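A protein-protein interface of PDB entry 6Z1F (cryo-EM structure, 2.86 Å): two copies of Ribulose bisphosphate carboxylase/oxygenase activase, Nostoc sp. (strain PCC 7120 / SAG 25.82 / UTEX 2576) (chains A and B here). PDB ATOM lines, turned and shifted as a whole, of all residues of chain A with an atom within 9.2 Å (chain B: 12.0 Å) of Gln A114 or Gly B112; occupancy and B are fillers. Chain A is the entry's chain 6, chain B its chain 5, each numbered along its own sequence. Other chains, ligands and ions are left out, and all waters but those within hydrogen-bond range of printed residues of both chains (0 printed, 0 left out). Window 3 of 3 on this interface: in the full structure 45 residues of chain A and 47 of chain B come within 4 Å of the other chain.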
ATOM      1  N   GLU A  66       2.048  -5.346  34.392  1.00  0.00           N
ATOM      2  CA  GLU A  66       1.473  -4.066  34.009  1.00  0.00           C
ATOM      3  C   GLU A  66       1.210  -3.227  35.255  1.00  0.00           C
ATOM      4  O   GLU A  66       0.236  -3.457  35.975  1.00  0.00           O
ATOM      5  CB  GLU A  66       0.236  -4.254  33.125  1.00  0.00           C
ATOM      6  CG  GLU A  66      -0.159  -3.001  32.352  1.00  0.00           C
ATOM      7  CD  GLU A  66       0.796  -2.529  31.263  1.00  0.00           C
ATOM      8  OE1 GLU A  66       1.285  -1.384  31.367  1.00  0.00           O
ATOM      9  OE2 GLU A  66       1.032  -3.293  30.302  1.00  0.00           O
ATOM     10  N   GLY A 107       0.490  -9.281  25.962  1.00  0.00           N
ATOM     11  CA  GLY A 107      -0.462  -9.594  24.907  1.00  0.00           C
ATOM     12  C   GLY A 107      -1.048  -8.347  24.248  1.00  0.00           C
ATOM     13  O   GLY A 107      -1.006  -7.260  24.824  1.00  0.00           O
ATOM     14  N   ARG A 108      -1.602  -8.534  23.040  1.00  0.00           N
ATOM     15  CA  ARG A 108      -2.215  -7.477  22.247  1.00  0.00           C
ATOM     16  C   ARG A 108      -3.393  -8.042  21.452  1.00  0.00           C
ATOM     17  O   ARG A 108      -3.215  -8.509  20.328  1.00  0.00           O
ATOM     18  CB  ARG A 108      -1.182  -6.870  21.292  1.00  0.00           C
ATOM     19  CG  ARG A 108      -0.262  -5.835  21.920  1.00  0.00           C
ATOM     20  CD  ARG A 108      -0.785  -4.422  21.753  1.00  0.00           C
ATOM     21  NE  ARG A 108      -0.319  -3.791  20.526  1.00  0.00           N
ATOM     22  CZ  ARG A 108       0.436  -2.696  20.459  1.00  0.00           C
ATOM     23  NH1 ARG A 108       0.795  -2.222  19.278  1.00  0.00           N
ATOM     24  NH2 ARG A 108       0.819  -2.067  21.558  1.00  0.00           N
ATOM     25  N   PHE A 109      -4.597  -7.972  22.038  1.00  0.00           N
ATOM     26  CA  PHE A 109      -5.796  -8.537  21.435  1.00  0.00           C
ATOM     27  C   PHE A 109      -6.360  -7.583  20.383  1.00  0.00           C
ATOM     28  O   PHE A 109      -5.765  -7.403  19.322  1.00  0.00           O
ATOM     29  CB  PHE A 109      -6.822  -8.914  22.509  1.00  0.00           C
ATOM     30  CG  PHE A 109      -6.391 -10.027  23.430  1.00  0.00           C
ATOM     31  CD1 PHE A 109      -6.550 -11.358  23.066  1.00  0.00           C
ATOM     32  CD2 PHE A 109      -5.819  -9.742  24.663  1.00  0.00           C
ATOM     33  CE1 PHE A 109      -6.146 -12.380  23.915  1.00  0.00           C
ATOM     34  CE2 PHE A 109      -5.417 -10.765  25.512  1.00  0.00           C
ATOM     35  CZ  PHE A 109      -5.582 -12.082  25.137  1.00  0.00           C
ATOM     36  N   ASP A 110      -7.516  -6.983  20.701  1.00  0.00           N
ATOM     37  CA  ASP A 110      -8.230  -6.068  19.824  1.00  0.00           C
ATOM     38  C   ASP A 110      -7.508  -4.721  19.786  1.00  0.00           C
ATOM     39  O   ASP A 110      -6.612  -4.464  20.590  1.00  0.00           O
ATOM     40  CB  ASP A 110      -9.702  -5.944  20.238  1.00  0.00           C
ATOM     41  CG  ASP A 110      -9.939  -5.422  21.650  1.00  0.00           C
ATOM     42  OD1 ASP A 110      -9.028  -5.544  22.497  1.00  0.00           O
ATOM     43  OD2 ASP A 110     -11.045  -4.900  21.897  1.00  0.00           O
ATOM     44  N   GLU A 111      -7.921  -3.868  18.840  1.00  0.00           N
ATOM     45  CA  GLU A 111      -7.377  -2.526  18.688  1.00  0.00           C
ATOM     46  C   GLU A 111      -8.254  -1.512  19.425  1.00  0.00           C
ATOM     47  O   GLU A 111      -7.984  -0.311  19.385  1.00  0.00           O
ATOM     48  CB  GLU A 111      -7.169  -2.190  17.206  1.00  0.00           C
ATOM     49  CG  GLU A 111      -8.439  -2.232  16.366  1.00  0.00           C
ATOM     50  CD  GLU A 111      -8.275  -1.960  14.879  1.00  0.00           C
ATOM     51  OE1 GLU A 111      -7.229  -1.402  14.481  1.00  0.00           O
ATOM     52  OE2 GLU A 111      -9.199  -2.306  14.117  1.00  0.00           O
ATOM     53  N   GLY A 112      -9.290  -2.014  20.111  1.00  0.00           N
ATOM     54  CA  GLY A 112     -10.237  -1.194  20.851  1.00  0.00           C
ATOM     55  C   GLY A 112      -9.739  -0.832  22.250  1.00  0.00           C
ATOM     56  O   GLY A 112     -10.374  -0.033  22.938  1.00  0.00           O
ATOM     57  N   THR A 113      -8.608  -1.425  22.653  1.00  0.00           N
ATOM     58  CA  THR A 113      -8.015  -1.212  23.967  1.00  0.00           C
ATOM     59  C   THR A 113      -6.858  -0.221  23.849  1.00  0.00           C
ATOM     60  O   THR A 113      -6.299  -0.039  22.768  1.00  0.00           O
ATOM     61  CB  THR A 113      -7.596  -2.545  24.606  1.00  0.00           C
ATOM     62  OG1 THR A 113      -8.591  -3.530  24.323  1.00  0.00           O
ATOM     63  CG2 THR A 113      -7.391  -2.460  26.104  1.00  0.00           C
ATOM     64  N   GLN A 114      -6.515   0.412  24.980  1.00  0.00           N
ATOM     65  CA  GLN A 114      -5.430   1.376  25.050  1.00  0.00           C
ATOM     66  C   GLN A 114      -4.248   0.754  25.789  1.00  0.00           C
ATOM     67  O   GLN A 114      -4.367   0.368  26.951  1.00  0.00           O
ATOM     68  CB  GLN A 114      -5.911   2.666  25.715  1.00  0.00           C
ATOM     69  CG  GLN A 114      -5.069   3.886  25.364  1.00  0.00           C
ATOM     70  CD  GLN A 114      -5.455   5.125  26.133  1.00  0.00           C
ATOM     71  OE1 GLN A 114      -6.589   5.285  26.583  1.00  0.00           O
ATOM     72  NE2 GLN A 114      -4.503   6.032  26.280  1.00  0.00           N
ATOM     73  N   TYR A 115      -3.113   0.675  25.086  1.00  0.00           N
ATOM     74  CA  TYR A 115      -1.891   0.078  25.600  1.00  0.00           C
ATOM     75  C   TYR A 115      -0.888   1.180  25.937  1.00  0.00           C
ATOM     76  O   TYR A 115      -1.114   2.347  25.621  1.00  0.00           O
ATOM     77  CB  TYR A 115      -1.331  -0.922  24.588  1.00  0.00           C
ATOM     78  CG  TYR A 115      -2.275  -2.032  24.199  1.00  0.00           C
ATOM     79  CD1 TYR A 115      -2.325  -3.215  24.923  1.00  0.00           C
ATOM     80  CD2 TYR A 115      -3.111  -1.908  23.097  1.00  0.00           C
ATOM     81  CE1 TYR A 115      -3.183  -4.245  24.568  1.00  0.00           C
ATOM     82  CE2 TYR A 115      -3.976  -2.927  22.728  1.00  0.00           C
ATOM     83  CZ  TYR A 115      -4.009  -4.101  23.465  1.00  0.00           C
ATOM     84  OH  TYR A 115      -4.856  -5.113  23.113  1.00  0.00           O
ATOM     85  N   THR A 116       0.226   0.787  26.571  1.00  0.00           N
ATOM     86  CA  THR A 116       1.237   1.704  27.074  1.00  0.00           C
ATOM     87  C   THR A 116       2.618   1.262  26.587  1.00  0.00           C
ATOM     88  O   THR A 116       2.729   0.348  25.771  1.00  0.00           O
ATOM     89  CB  THR A 116       1.121   1.816  28.603  1.00  0.00           C
ATOM     90  OG1 THR A 116      -0.246   2.038  28.951  1.00  0.00           O
ATOM     91  CG2 THR A 116       1.969   2.913  29.209  1.00  0.00           C
ATOM     92  N   VAL A 117       3.666   1.921  27.104  1.00  0.00           N
ATOM     93  CA  VAL A 117       5.062   1.636  26.799  1.00  0.00           C
ATOM     94  C   VAL A 117       5.452   0.255  27.322  1.00  0.00           C
ATOM     95  O   VAL A 117       6.385  -0.354  26.804  1.00  0.00           O
ATOM     96  CB  VAL A 117       6.022   2.707  27.361  1.00  0.00           C
ATOM     97  CG1 VAL A 117       5.927   4.022  26.617  1.00  0.00           C
ATOM     98  CG2 VAL A 117       5.863   2.928  28.859  1.00  0.00           C
ATOM     99  N   THR A 119       4.029  -2.705  27.398  1.00  0.00           N
ATOM    100  CA  THR A 119       3.787  -3.821  26.493  1.00  0.00           C
ATOM    101  C   THR A 119       4.991  -4.002  25.567  1.00  0.00           C
ATOM    102  O   THR A 119       5.452  -5.118  25.341  1.00  0.00           O
ATOM    103  CB  THR A 119       2.495  -3.599  25.692  1.00  0.00           C
ATOM    104  OG1 THR A 119       1.466  -3.160  26.580  1.00  0.00           O
ATOM    105  CG2 THR A 119       2.035  -4.834  24.948  1.00  0.00           C
ATOM    106  N   GLY B 107      10.898   3.783  19.909  1.00  0.00           N
ATOM    107  CA  GLY B 107       9.974   3.680  18.792  1.00  0.00           C
ATOM    108  C   GLY B 107       8.517   3.791  19.230  1.00  0.00           C
ATOM    109  O   GLY B 107       8.198   3.549  20.393  1.00  0.00           O
ATOM    110  N   ARG B 108       7.655   4.156  18.272  1.00  0.00           N
ATOM    111  CA  ARG B 108       6.230   4.334  18.506  1.00  0.00           C
ATOM    112  C   ARG B 108       5.443   3.436  17.557  1.00  0.00           C
ATOM    113  O   ARG B 108       5.408   3.692  16.356  1.00  0.00           O
ATOM    114  CB  ARG B 108       5.827   5.799  18.319  1.00  0.00           C
ATOM    115  CG  ARG B 108       6.641   6.785  19.142  1.00  0.00           C
ATOM    116  CD  ARG B 108       5.930   8.116  19.244  1.00  0.00           C
ATOM    117  NE  ARG B 108       6.668   9.033  20.102  1.00  0.00           N
ATOM    118  CZ  ARG B 108       6.121   9.960  20.882  1.00  0.00           C
ATOM    119  NH1 ARG B 108       6.895  10.737  21.620  1.00  0.00           N
ATOM    120  NH2 ARG B 108       4.806  10.106  20.936  1.00  0.00           N
ATOM    121  N   PHE B 109       4.796   2.408  18.122  1.00  0.00           N
ATOM    122  CA  PHE B 109       4.111   1.373  17.361  1.00  0.00           C
ATOM    123  C   PHE B 109       2.936   1.959  16.585  1.00  0.00           C
ATOM    124  O   PHE B 109       2.924   1.911  15.354  1.00  0.00           O
ATOM    125  CB  PHE B 109       3.671   0.232  18.283  1.00  0.00           C
ATOM    126  CG  PHE B 109       4.705  -0.836  18.544  1.00  0.00           C
ATOM    127  CD1 PHE B 109       6.061  -0.530  18.622  1.00  0.00           C
ATOM    128  CD2 PHE B 109       4.317  -2.155  18.746  1.00  0.00           C
ATOM    129  CE1 PHE B 109       7.003  -1.520  18.871  1.00  0.00           C
ATOM    130  CE2 PHE B 109       5.259  -3.144  19.001  1.00  0.00           C
ATOM    131  CZ  PHE B 109       6.600  -2.825  19.063  1.00  0.00           C
ATOM    132  N   ASP B 110       1.957   2.511  17.313  1.00  0.00           N
ATOM    133  CA  ASP B 110       0.765   3.084  16.708  1.00  0.00           C
ATOM    134  C   ASP B 110       0.608   4.538  17.154  1.00  0.00           C
ATOM    135  O   ASP B 110       1.466   5.075  17.853  1.00  0.00           O
ATOM    136  CB  ASP B 110      -0.471   2.208  16.958  1.00  0.00           C
ATOM    137  CG  ASP B 110      -1.013   2.216  18.382  1.00  0.00           C
ATOM    138  OD1 ASP B 110      -0.368   2.813  19.266  1.00  0.00           O
ATOM    139  OD2 ASP B 110      -2.087   1.618  18.597  1.00  0.00           O
ATOM    140  N   GLU B 111      -0.506   5.154  16.738  1.00  0.00           N
ATOM    141  CA  GLU B 111      -0.854   6.516  17.112  1.00  0.00           C
ATOM    142  C   GLU B 111      -1.971   6.475  18.157  1.00  0.00           C
ATOM    143  O   GLU B 111      -2.844   7.342  18.188  1.00  0.00           O
ATOM    144  CB  GLU B 111      -1.189   7.313  15.846  1.00  0.00           C
ATOM    145  CG  GLU B 111      -1.328   8.820  16.045  1.00  0.00           C
ATOM    146  CD  GLU B 111      -0.178   9.565  16.710  1.00  0.00           C
ATOM    147  OE1 GLU B 111       0.993   9.266  16.393  1.00  0.00           O
ATOM    148  OE2 GLU B 111      -0.458  10.452  17.543  1.00  0.00           O
ATOM    149  N   GLY B 112      -1.924   5.458  19.026  1.00  0.00           N
ATOM    150  CA  GLY B 112      -2.911   5.280  20.079  1.00  0.00           C
ATOM    151  C   GLY B 112      -2.277   4.919  21.420  1.00  0.00           C
ATOM    152  O   GLY B 112      -2.966   4.893  22.438  1.00  0.00           O
ATOM    153  N   THR B 113      -0.965   4.646  21.402  1.00  0.00           N
ATOM    154  CA  THR B 113      -0.232   4.226  22.584  1.00  0.00           C
ATOM    155  C   THR B 113       0.254   5.452  23.351  1.00  0.00           C
ATOM    156  O   THR B 113       0.856   6.354  22.771  1.00  0.00           O
ATOM    157  CB  THR B 113       0.913   3.271  22.221  1.00  0.00           C
ATOM    158  OG1 THR B 113       0.334   2.126  21.598  1.00  0.00           O
ATOM    159  CG2 THR B 113       1.716   2.817  23.418  1.00  0.00           C
ATOM    160  N   GLN B 114      -0.021   5.453  24.661  1.00  0.00           N
ATOM    161  CA  GLN B 114       0.432   6.488  25.576  1.00  0.00           C
ATOM    162  C   GLN B 114       1.924   6.285  25.841  1.00  0.00           C
ATOM    163  O   GLN B 114       2.338   5.212  26.274  1.00  0.00           O
ATOM    164  CB  GLN B 114      -0.441   6.462  26.833  1.00  0.00           C
ATOM    165  CG  GLN B 114      -0.076   7.512  27.871  1.00  0.00           C
ATOM    166  CD  GLN B 114       0.885   7.005  28.919  1.00  0.00           C
ATOM    167  OE1 GLN B 114       0.940   5.816  29.225  1.00  0.00           O
ATOM    168  NE2 GLN B 114       1.644   7.920  29.501  1.00  0.00           N
ATOM    169  N   TYR B 115       2.716   7.325  25.550  1.00  0.00           N
ATOM    170  CA  TYR B 115       4.151   7.334  25.796  1.00  0.00           C
ATOM    171  C   TYR B 115       4.495   8.369  26.866  1.00  0.00           C
ATOM    172  O   TYR B 115       3.660   9.193  27.237  1.00  0.00           O
ATOM    173  CB  TYR B 115       4.919   7.596  24.496  1.00  0.00           C
ATOM    174  CG  TYR B 115       5.055   6.385  23.612  1.00  0.00           C
ATOM    175  CD1 TYR B 115       6.153   5.548  23.726  1.00  0.00           C
ATOM    176  CD2 TYR B 115       4.082   6.062  22.677  1.00  0.00           C
ATOM    177  CE1 TYR B 115       6.279   4.410  22.942  1.00  0.00           C
ATOM    178  CE2 TYR B 115       4.199   4.937  21.874  1.00  0.00           C
ATOM    179  CZ  TYR B 115       5.299   4.107  22.012  1.00  0.00           C
ATOM    180  OH  TYR B 115       5.408   2.999  21.224  1.00  0.00           O
ATOM    181  N   THR B 116       5.744   8.313  27.344  1.00  0.00           N
ATOM    182  CA  THR B 116       6.256   9.249  28.334  1.00  0.00           C
ATOM    183  C   THR B 116       7.268  10.193  27.688  1.00  0.00           C
ATOM    184  O   THR B 116       7.354  10.288  26.465  1.00  0.00           O
ATOM    185  CB  THR B 116       6.900   8.516  29.518  1.00  0.00           C
ATOM    186  OG1 THR B 116       8.008   7.765  29.024  1.00  0.00           O
ATOM    187  CG2 THR B 116       5.933   7.625  30.266  1.00  0.00           C
ATOM    188  N   THR B 161       9.431   3.583  12.515  1.00  0.00           N
ATOM    189  CA  THR B 161       8.832   4.072  13.746  1.00  0.00           C
ATOM    190  C   THR B 161       9.942   4.592  14.655  1.00  0.00           C
ATOM    191  O   THR B 161      10.268   3.964  15.659  1.00  0.00           O
ATOM    192  CB  THR B 161       7.977   2.987  14.417  1.00  0.00           C
ATOM    193  OG1 THR B 161       8.805   1.850  14.672  1.00  0.00           O
ATOM    194  CG2 THR B 161       6.771   2.579  13.596  1.00  0.00           C
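Gln A114 touches one residue of chain B.
Gly B112 touches just one residue of chain A: Gln A114.
No residue of chain B comes within 4 Å of Gly A112.
No residue of chain B comes within 4 Å of Thr A113.
Tyr A115 touches just these residues of chain B: Thr B113 (3.6 Å) and Gln B114 (3.4 Å).
Thr A116 touches just these residues of chain B: Thr B113 (3.6 Å) and Gln B114 (3.1 Å).
Printed residues of chain B within 4 Å of Arg A108: Phe B109 (3.6 Å).
Of the printed residues of chain A, Phe B109 touches Arg A108.
Of the printed residues of chain B, Val A117 touches Gln B114 (3.6 Å) and Tyr B115 (3.3 Å).
Printed residues of chain A within 4 Å of Tyr B115: Val A117.
The nearest residue of chain B that does not touch Gln A114 is Gln B114 (4.1 Å).
The nearest residue of chain A that does not touch Gly B112 is Tyr A115 (4.5 Å).
NH1 of Arg A108 touches CD2 of Phe B109 (3.6 Å).
CG of Gln A114 touches O of Gly B112, 3.7 Å away.
Thr B113 touches Tyr A115 (CG2 to O, 3.6 Å).
Thr A116 touches Thr B113.
Gln B114 touches Thr A116.
Val A117 touches Gln B114.
Tyr B115 touches Val A117 (CD1 to CG1, 3.3 Å).
The backbone carbonyl oxygen of Tyr A115 lies within hydrogen-bond range of the backbone NH of Gln B114, 3.4 Å away.
Hydrophobic or aromatic side chains of chain A that line the printed part of chain B: Val A117.
Hydrophobic or aromatic side chains of chain B within 4 Å of the printed part of chain A: Phe B109 and Tyr B115.
Arg A108 touches Phe B109, but with the chains exchanged Phe A109 does not touch Arg B108 (15.7 Å).
Gln A114 touches Gly B112, but with the chains exchanged Gly A112 does not touch Gln B114 (11.8 Å).
Tyr A115 touches Thr B113, but with the chains exchanged Thr A113 does not touch Tyr B115 (11.7 Å).
Tyr A115 touches Gln B114, but with the chains exchanged Gln A114 does not touch Tyr B115 (7.4 Å).
Positions printed for both chains: 107, 108, 109, 110, 111, 112, 113, 114, 115 and 116.
O of Gly B107 is in hydrogen-bond range of OH of Tyr B115, 3.0 Å away.
The backbone NH (N) of Phe B109 is in hydrogen-bond range of the side-chain hydroxyl (OH) of Tyr B115, at 3.2 Å.
The side-chain carboxylate (OD1) of Asp B110 is in hydrogen-bond range of the backbone NH (N) of Gly B112, 3.1 Å away.
OD1 of Asp B110 lies within hydrogen-bond range of OG1 of Thr B113 (2.5 Å).
The side-chain hydroxyl (OH) of Tyr A115 lies within hydrogen-bond range of the backbone NH (N) of Phe A109 (3.1 Å).
OH of Tyr A115 is in hydrogen-bond range of O of Asp A110 (3.1 Å).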
